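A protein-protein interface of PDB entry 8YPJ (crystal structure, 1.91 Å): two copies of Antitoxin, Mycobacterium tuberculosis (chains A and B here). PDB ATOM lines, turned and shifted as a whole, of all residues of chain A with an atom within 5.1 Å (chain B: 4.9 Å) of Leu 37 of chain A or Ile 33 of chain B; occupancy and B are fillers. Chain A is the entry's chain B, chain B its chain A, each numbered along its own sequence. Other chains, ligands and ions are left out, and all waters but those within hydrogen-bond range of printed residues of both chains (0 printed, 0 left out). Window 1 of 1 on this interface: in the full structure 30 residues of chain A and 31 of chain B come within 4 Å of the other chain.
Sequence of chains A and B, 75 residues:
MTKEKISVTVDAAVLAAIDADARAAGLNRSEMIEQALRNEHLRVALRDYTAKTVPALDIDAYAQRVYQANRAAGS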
ATOM      1  N   ILE A   6      11.699  24.022  22.616  1.00  0.00           N
ATOM      2  CA  ILE A   6      12.160  23.620  23.936  1.00  0.00           C
ATOM      3  C   ILE A   6      13.136  24.628  24.502  1.00  0.00           C
ATOM      4  O   ILE A   6      13.658  25.472  23.783  1.00  0.00           O
ATOM      5  CB  ILE A   6      12.853  22.251  23.898  1.00  0.00           C
ATOM      6  CG1 ILE A   6      14.152  22.344  23.088  1.00  0.00           C
ATOM      7  CG2 ILE A   6      11.933  21.198  23.302  1.00  0.00           C
ATOM      8  CD1 ILE A   6      14.895  21.037  22.983  1.00  0.00           C
ATOM      9  N   VAL A   8      16.783  24.779  26.629  1.00  0.00           N
ATOM     10  CA  VAL A   8      17.911  23.984  27.069  1.00  0.00           C
ATOM     11  C   VAL A   8      18.949  24.888  27.712  1.00  0.00           C
ATOM     12  O   VAL A   8      18.995  26.081  27.450  1.00  0.00           O
ATOM     13  CB  VAL A   8      18.543  23.195  25.907  1.00  0.00           C
ATOM     14  CG1 VAL A   8      17.535  22.215  25.325  1.00  0.00           C
ATOM     15  CG2 VAL A   8      19.030  24.140  24.834  1.00  0.00           C
ATOM     16  N   VAL A  10      22.939  25.401  28.228  1.00  0.00           N
ATOM     17  CA  VAL A  10      24.197  24.914  27.678  1.00  0.00           C
ATOM     18  C   VAL A  10      25.386  25.827  27.997  1.00  0.00           C
ATOM     19  O   VAL A  10      25.224  27.020  28.215  1.00  0.00           O
ATOM     20  CB  VAL A  10      24.090  24.720  26.136  1.00  0.00           C
ATOM     21  CG1 VAL A  10      23.137  23.560  25.803  1.00  0.00           C
ATOM     22  CG2 VAL A  10      23.618  25.995  25.473  1.00  0.00           C
ATOM     23  N   ILE A  33      21.451  23.574  15.360  1.00  0.00           N
ATOM     24  CA  ILE A  33      21.337  22.693  16.514  1.00  0.00           C
ATOM     25  C   ILE A  33      20.671  21.395  16.083  1.00  0.00           C
ATOM     26  O   ILE A  33      21.105  20.312  16.475  1.00  0.00           O
ATOM     27  CB  ILE A  33      20.581  23.381  17.670  1.00  0.00           C
ATOM     28  CG1 ILE A  33      21.538  24.389  18.327  1.00  0.00           C
ATOM     29  CG2 ILE A  33      20.094  22.354  18.701  1.00  0.00           C
ATOM     30  CD1 ILE A  33      20.992  25.148  19.503  1.00  0.00           C
ATOM     31  N   GLU A  34      19.655  21.492  15.237  1.00  0.00           N
ATOM     32  CA  GLU A  34      19.014  20.278  14.722  1.00  0.00           C
ATOM     33  C   GLU A  34      19.987  19.432  13.912  1.00  0.00           C
ATOM     34  O   GLU A  34      19.987  18.207  14.011  1.00  0.00           O
ATOM     35  CB  GLU A  34      17.796  20.620  13.864  1.00  0.00           C
ATOM     36  CG  GLU A  34      17.032  19.378  13.424  1.00  0.00           C
ATOM     37  CD  GLU A  34      15.708  19.696  12.743  1.00  0.00           C
ATOM     38  OE1 GLU A  34      14.847  20.358  13.371  1.00  0.00           O
ATOM     39  OE2 GLU A  34      15.536  19.275  11.576  1.00  0.00           O
ATOM     40  N   GLN A  35      20.803  20.081  13.087  1.00  0.00           N
ATOM     41  CA  GLN A  35      21.865  19.368  12.388  1.00  0.00           C
ATOM     42  C   GLN A  35      22.798  18.646  13.371  1.00  0.00           C
ATOM     43  O   GLN A  35      23.127  17.467  13.196  1.00  0.00           O
ATOM     44  CB  GLN A  35      22.664  20.335  11.508  1.00  0.00           C
ATOM     45  CG  GLN A  35      23.827  19.676  10.794  1.00  0.00           C
ATOM     46  CD  GLN A  35      24.529  20.631   9.844  1.00  0.00           C
ATOM     47  OE1 GLN A  35      23.917  21.153   8.911  1.00  0.00           O
ATOM     48  NE2 GLN A  35      25.816  20.862  10.076  1.00  0.00           N
ATOM     49  N   ALA A  36      23.235  19.357  14.401  1.00  0.00           N
ATOM     50  CA  ALA A  36      24.079  18.753  15.439  1.00  0.00           C
ATOM     51  C   ALA A  36      23.435  17.502  16.045  1.00  0.00           C
ATOM     52  O   ALA A  36      24.083  16.475  16.238  1.00  0.00           O
ATOM     53  CB  ALA A  36      24.369  19.765  16.539  1.00  0.00           C
ATOM     54  N   LEU A  37      22.157  17.603  16.360  1.00  0.00           N
ATOM     55  CA  LEU A  37      21.448  16.488  16.994  1.00  0.00           C
ATOM     56  C   LEU A  37      21.279  15.285  16.056  1.00  0.00           C
ATOM     57  O   LEU A  37      21.464  14.135  16.464  1.00  0.00           O
ATOM     58  CB  LEU A  37      20.076  16.967  17.481  1.00  0.00           C
ATOM     59  CG  LEU A  37      20.109  18.117  18.488  1.00  0.00           C
ATOM     60  CD1 LEU A  37      18.707  18.407  19.011  1.00  0.00           C
ATOM     61  CD2 LEU A  37      21.063  17.804  19.617  1.00  0.00           C
ATOM     62  N   ARG A  38      20.899  15.547  14.810  1.00  0.00           N
ATOM     63  CA  ARG A  38      20.801  14.481  13.810  1.00  0.00           C
ATOM     64  C   ARG A  38      22.119  13.717  13.684  1.00  0.00           C
ATOM     65  O   ARG A  38      22.146  12.488  13.711  1.00  0.00           O
ATOM     66  CB  ARG A  38      20.409  15.054  12.450  1.00  0.00           C
ATOM     67  CG  ARG A  38      18.953  15.474  12.333  1.00  0.00           C
ATOM     68  CD  ARG A  38      18.588  15.705  10.864  1.00  0.00           C
ATOM     69  NE  ARG A  38      18.306  17.110  10.578  1.00  0.00           N
ATOM     70  CZ  ARG A  38      19.153  17.953   9.986  1.00  0.00           C
ATOM     71  NH1 ARG A  38      20.354  17.540   9.600  1.00  0.00           N
ATOM     72  NH2 ARG A  38      18.795  19.216   9.775  1.00  0.00           N
ATOM     73  N   ASN A  39      23.219  14.454  13.526  1.00  0.00           N
ATOM     74  CA  ASN A  39      24.525  13.823  13.383  1.00  0.00           C
ATOM     75  C   ASN A  39      24.954  13.118  14.649  1.00  0.00           C
ATOM     76  O   ASN A  39      25.570  12.060  14.595  1.00  0.00           O
ATOM     77  CB  ASN A  39      25.590  14.852  12.976  1.00  0.00           C
ATOM     78  CG  ASN A  39      25.343  15.415  11.586  1.00  0.00           C
ATOM     79  OD1 ASN A  39      24.610  14.825  10.785  1.00  0.00           O
ATOM     80  ND2 ASN A  39      25.942  16.558  11.296  1.00  0.00           N
ATOM     81  N   GLU A  40      24.661  13.703  15.804  1.00  0.00           N
ATOM     82  CA  GLU A  40      25.104  13.045  17.030  1.00  0.00           C
ATOM     83  C   GLU A  40      24.308  11.759  17.264  1.00  0.00           C
ATOM     84  O   GLU A  40      24.843  10.783  17.789  1.00  0.00           O
ATOM     85  CB  GLU A  40      24.963  13.962  18.251  1.00  0.00           C
ATOM     86  CG  GLU A  40      25.655  13.410  19.497  1.00  0.00           C
ATOM     87  CD  GLU A  40      27.173  13.355  19.367  1.00  0.00           C
ATOM     88  OE1 GLU A  40      27.744  14.052  18.490  1.00  0.00           O
ATOM     89  OE2 GLU A  40      27.802  12.598  20.142  1.00  0.00           O
ATOM     90  N   HIS A  41      23.028  11.764  16.901  1.00  0.00           N
ATOM     91  CA  HIS A  41      22.227  10.551  17.079  1.00  0.00           C
ATOM     92  C   HIS A  41      22.823   9.397  16.258  1.00  0.00           C
ATOM     93  O   HIS A  41      22.983   8.278  16.757  1.00  0.00           O
ATOM     94  CB  HIS A  41      20.774  10.784  16.684  1.00  0.00           C
ATOM     95  CG  HIS A  41      19.936   9.549  16.777  1.00  0.00           C
ATOM     96  ND1 HIS A  41      19.789   8.841  17.953  1.00  0.00           N
ATOM     97  CD2 HIS A  41      19.228   8.878  15.839  1.00  0.00           C
ATOM     98  CE1 HIS A  41      19.016   7.789  17.734  1.00  0.00           C
ATOM     99  NE2 HIS A  41      18.658   7.792  16.462  1.00  0.00           N
ATOM    100  N   LEU A  42      23.171   9.672  15.006  1.00  0.00           N
ATOM    101  CA  LEU A  42      23.804   8.645  14.178  1.00  0.00           C
ATOM    102  C   LEU A  42      25.152   8.217  14.758  1.00  0.00           C
ATOM    103  O   LEU A  42      25.483   7.037  14.772  1.00  0.00           O
ATOM    104  CB  LEU A  42      23.965   9.135  12.740  1.00  0.00           C
ATOM    105  CG  LEU A  42      24.548   8.097  11.769  1.00  0.00           C
ATOM    106  CD1 LEU A  42      23.716   6.803  11.757  1.00  0.00           C
ATOM    107  CD2 LEU A  42      24.647   8.689  10.378  1.00  0.00           C
ATOM    108  N   VAL B  10      13.100  22.412  17.268  1.00  0.00           N
ATOM    109  CA  VAL B  10      13.696  21.266  16.592  1.00  0.00           C
ATOM    110  C   VAL B  10      12.670  20.177  16.249  1.00  0.00           C
ATOM    111  O   VAL B  10      11.624  20.063  16.888  1.00  0.00           O
ATOM    112  CB  VAL B  10      14.828  20.642  17.449  1.00  0.00           C
ATOM    113  CG1 VAL B  10      15.969  21.648  17.664  1.00  0.00           C
ATOM    114  CG2 VAL B  10      14.287  20.155  18.781  1.00  0.00           C
ATOM    115  N   VAL B  14      13.622  13.956  16.052  1.00  0.00           N
ATOM    116  CA  VAL B  14      15.021  14.118  16.427  1.00  0.00           C
ATOM    117  C   VAL B  14      15.134  14.270  17.939  1.00  0.00           C
ATOM    118  O   VAL B  14      15.997  13.670  18.575  1.00  0.00           O
ATOM    119  CB  VAL B  14      15.649  15.332  15.712  1.00  0.00           C
ATOM    120  CG1 VAL B  14      17.092  15.545  16.155  1.00  0.00           C
ATOM    121  CG2 VAL B  14      15.579  15.129  14.198  1.00  0.00           C
ATOM    122  N   ILE B  18      17.217  11.954  20.684  1.00  0.00           N
ATOM    123  CA  ILE B  18      18.252  12.538  21.538  1.00  0.00           C
ATOM    124  C   ILE B  18      17.905  12.287  23.018  1.00  0.00           C
ATOM    125  O   ILE B  18      18.785  12.023  23.831  1.00  0.00           O
ATOM    126  CB  ILE B  18      18.407  14.045  21.245  1.00  0.00           C
ATOM    127  CG1 ILE B  18      19.231  14.241  19.964  1.00  0.00           C
ATOM    128  CG2 ILE B  18      19.081  14.768  22.401  1.00  0.00           C
ATOM    129  CD1 ILE B  18      20.658  13.673  20.037  1.00  0.00           C
ATOM    130  N   ARG B  29      18.657  15.937  29.154  1.00  0.00           N
ATOM    131  CA  ARG B  29      18.561  16.437  27.787  1.00  0.00           C
ATOM    132  C   ARG B  29      19.568  17.550  27.482  1.00  0.00           C
ATOM    133  O   ARG B  29      20.192  17.549  26.420  1.00  0.00           O
ATOM    134  CB  ARG B  29      17.151  16.940  27.504  1.00  0.00           C
ATOM    135  CG  ARG B  29      16.991  17.438  26.070  1.00  0.00           C
ATOM    136  CD  ARG B  29      15.651  18.101  25.858  1.00  0.00           C
ATOM    137  NE  ARG B  29      14.578  17.130  25.682  1.00  0.00           N
ATOM    138  CZ  ARG B  29      13.288  17.452  25.667  1.00  0.00           C
ATOM    139  NH1 ARG B  29      12.917  18.721  25.826  1.00  0.00           N
ATOM    140  NH2 ARG B  29      12.366  16.510  25.502  1.00  0.00           N
ATOM    141  N   SER B  30      19.727  18.506  28.400  1.00  0.00           N
ATOM    142  CA  SER B  30      20.686  19.596  28.172  1.00  0.00           C
ATOM    143  C   SER B  30      22.131  19.124  28.010  1.00  0.00           C
ATOM    144  O   SER B  30      22.858  19.632  27.145  1.00  0.00           O
ATOM    145  CB  SER B  30      20.617  20.624  29.313  1.00  0.00           C
ATOM    146  OG  SER B  30      19.438  21.391  29.196  1.00  0.00           O
ATOM    147  N   GLU B  31      22.562  18.182  28.851  1.00  0.00           N
ATOM    148  CA  GLU B  31      23.911  17.615  28.750  1.00  0.00           C
ATOM    149  C   GLU B  31      24.140  16.882  27.413  1.00  0.00           C
ATOM    150  O   GLU B  31      25.200  17.020  26.789  1.00  0.00           O
ATOM    151  CB  GLU B  31      24.184  16.655  29.932  1.00  0.00           C
ATOM    152  CG  GLU B  31      24.214  17.346  31.310  1.00  0.00           C
ATOM    153  CD  GLU B  31      24.070  16.377  32.486  1.00  0.00           C
ATOM    154  OE1 GLU B  31      23.520  15.267  32.289  1.00  0.00           O
ATOM    155  OE2 GLU B  31      24.501  16.731  33.617  1.00  0.00           O
ATOM    156  N   MET B  32      23.155  16.102  26.975  1.00  0.00           N
ATOM    157  CA  MET B  32      23.279  15.366  25.710  1.00  0.00           C
ATOM    158  C   MET B  32      23.319  16.336  24.531  1.00  0.00           C
ATOM    159  O   MET B  32      24.092  16.167  23.591  1.00  0.00           O
ATOM    160  CB  MET B  32      22.116  14.385  25.538  1.00  0.00           C
ATOM    161  CG  MET B  32      22.225  13.486  24.304  1.00  0.00           C
ATOM    162  SD  MET B  32      23.607  12.309  24.407  1.00  0.00           S
ATOM    163  CE  MET B  32      24.179  12.411  22.720  1.00  0.00           C
ATOM    164  N   ILE B  33      22.498  17.377  24.597  1.00  0.00           N
ATOM    165  CA  ILE B  33      22.501  18.365  23.524  1.00  0.00           C
ATOM    166  C   ILE B  33      23.856  19.093  23.495  1.00  0.00           C
ATOM    167  O   ILE B  33      24.435  19.328  22.426  1.00  0.00           O
ATOM    168  CB  ILE B  33      21.327  19.349  23.680  1.00  0.00           C
ATOM    169  CG1 ILE B  33      20.024  18.608  23.355  1.00  0.00           C
ATOM    170  CG2 ILE B  33      21.529  20.566  22.760  1.00  0.00           C
ATOM    171  CD1 ILE B  33      18.746  19.423  23.474  1.00  0.00           C
ATOM    172  N   GLU B  34      24.385  19.414  24.667  1.00  0.00           N
ATOM    173  CA  GLU B  34      25.703  20.049  24.733  1.00  0.00           C
ATOM    174  C   GLU B  34      26.782  19.159  24.119  1.00  0.00           C
ATOM    175  O   GLU B  34      27.644  19.641  23.375  1.00  0.00           O
ATOM    176  CB  GLU B  34      26.070  20.411  26.178  1.00  0.00           C
ATOM    177  CG  GLU B  34      27.421  21.133  26.286  1.00  0.00           C
ATOM    178  CD  GLU B  34      27.758  21.579  27.702  1.00  0.00           C
ATOM    179  OE1 GLU B  34      26.928  22.281  28.325  1.00  0.00           O
ATOM    180  OE2 GLU B  34      28.865  21.244  28.173  1.00  0.00           O
ATOM    181  N   GLN B  35      26.740  17.862  24.406  1.00  0.00           N
ATOM    182  CA  GLN B  35      27.673  16.937  23.768  1.00  0.00           C
ATOM    183  C   GLN B  35      27.556  16.995  22.241  1.00  0.00           C
ATOM    184  O   GLN B  35      28.571  17.026  21.550  1.00  0.00           O
ATOM    185  CB  GLN B  35      27.448  15.490  24.257  1.00  0.00           C
ATOM    186  CG  GLN B  35      28.168  14.422  23.408  1.00  0.00           C
ATOM    187  CD  GLN B  35      27.930  12.995  23.899  1.00  0.00           C
ATOM    188  OE1 GLN B  35      28.033  12.719  25.087  1.00  0.00           O
ATOM    189  NE2 GLN B  35      27.622  12.083  22.972  1.00  0.00           N
ATOM    190  N   ALA B  36      26.322  16.996  21.731  1.00  0.00           N
ATOM    191  CA  ALA B  36      26.055  17.056  20.297  1.00  0.00           C
ATOM    192  C   ALA B  36      26.641  18.332  19.695  1.00  0.00           C
ATOM    193  O   ALA B  36      27.251  18.297  18.622  1.00  0.00           O
ATOM    194  CB  ALA B  36      24.554  16.999  20.028  1.00  0.00           C
ATOM    195  N   LEU B  37      26.463  19.450  20.397  1.00  0.00           N
ATOM    196  CA  LEU B  37      26.940  20.749  19.898  1.00  0.00           C
ATOM    197  C   LEU B  37      28.466  20.830  19.898  1.00  0.00           C
ATOM    198  O   LEU B  37      29.070  21.362  18.964  1.00  0.00           O
ATOM    199  CB  LEU B  37      26.361  21.900  20.733  1.00  0.00           C
ATOM    200  CG  LEU B  37      24.839  22.062  20.825  1.00  0.00           C
ATOM    201  CD1 LEU B  37      24.478  23.342  21.598  1.00  0.00           C
ATOM    202  CD2 LEU B  37      24.212  22.080  19.451  1.00  0.00           C
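Val 10 of chain A touches Glu 34 of chain B, and with the chains exchanged Glu 34 of chain A touches Val 10 of chain B. Ile 33 of chain A touches Leu 37 of chain B, and with the chains exchanged Leu 37 of chain A touches Ile 33 of chain B. Ala 36 of chain A touches its own counterpart, Ala 36 of chain B. Ala 36 of chain A touches Leu 37 of chain B, and with the chains exchanged Leu 37 of chain A touches Ala 36 of chain B. Of the 16 pairs that touch across the chains among the printed residues, 7 have their exchanged pair printed and touching as well.
NE2 of Gln 35 of chain B lies within hydrogen-bond range of OE2 of Glu 40 of chain A, 2.9 Å away.
Among the printed residues, 16 pairs touch across the chains. Among the printed residues, no Asp or Glu carboxylate lies within 4 Å of a Lys or Arg side-chain nitrogen of the other chain.
OE1 of Glu 34 of chain B touches CA of Val 10 of chain A (3.8 Å). Leu 37 of chain B touches Ile 33 of chain A. CB of Ala 36 of chain A touches O of Ala 36 of chain B (3.8 Å). Ala 36 of chain A touches Leu 37 of chain B. Leu 37 of chain A touches Val 14 of chain B. O of Leu 37 of chain A touches CD1 of Ile 18 of chain B (3.7 Å). CD2 of Leu 37 of chain A touches CG1 of Ile 33 of chain B, 3.96 Å away. Val 14 of chain B touches Arg 38 of chain A (CG2 to CG, 3.9 Å). CG of Glu 40 of chain A touches CE of Met 32 of chain B, 3.7 Å away. Ala 36 of chain B touches Glu 40 of chain A (CB to CB, 3.5 Å).
The side-chain carboxylate (OE2) of Glu 34 of chain A lies within salt-bridge range of the guanidinium group (NE) of Arg 38 of chain A, at 3.7 Å.
Gln 35 of chain A touches none of the printed residues of chain B. Of the printed residues of chain B, Ala 36 of chain A touches Ala 36 (3.8 Å) and Leu 37 (3.7 Å). Leu 37 of chain A touches four residues of chain B. His 41 of chain A touches none of the printed residues of chain B. Of the printed residues of chain A, Val 10 of chain B touches Glu 34. Of the printed residues of chain A, Met 32 of chain B touches Glu 40.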
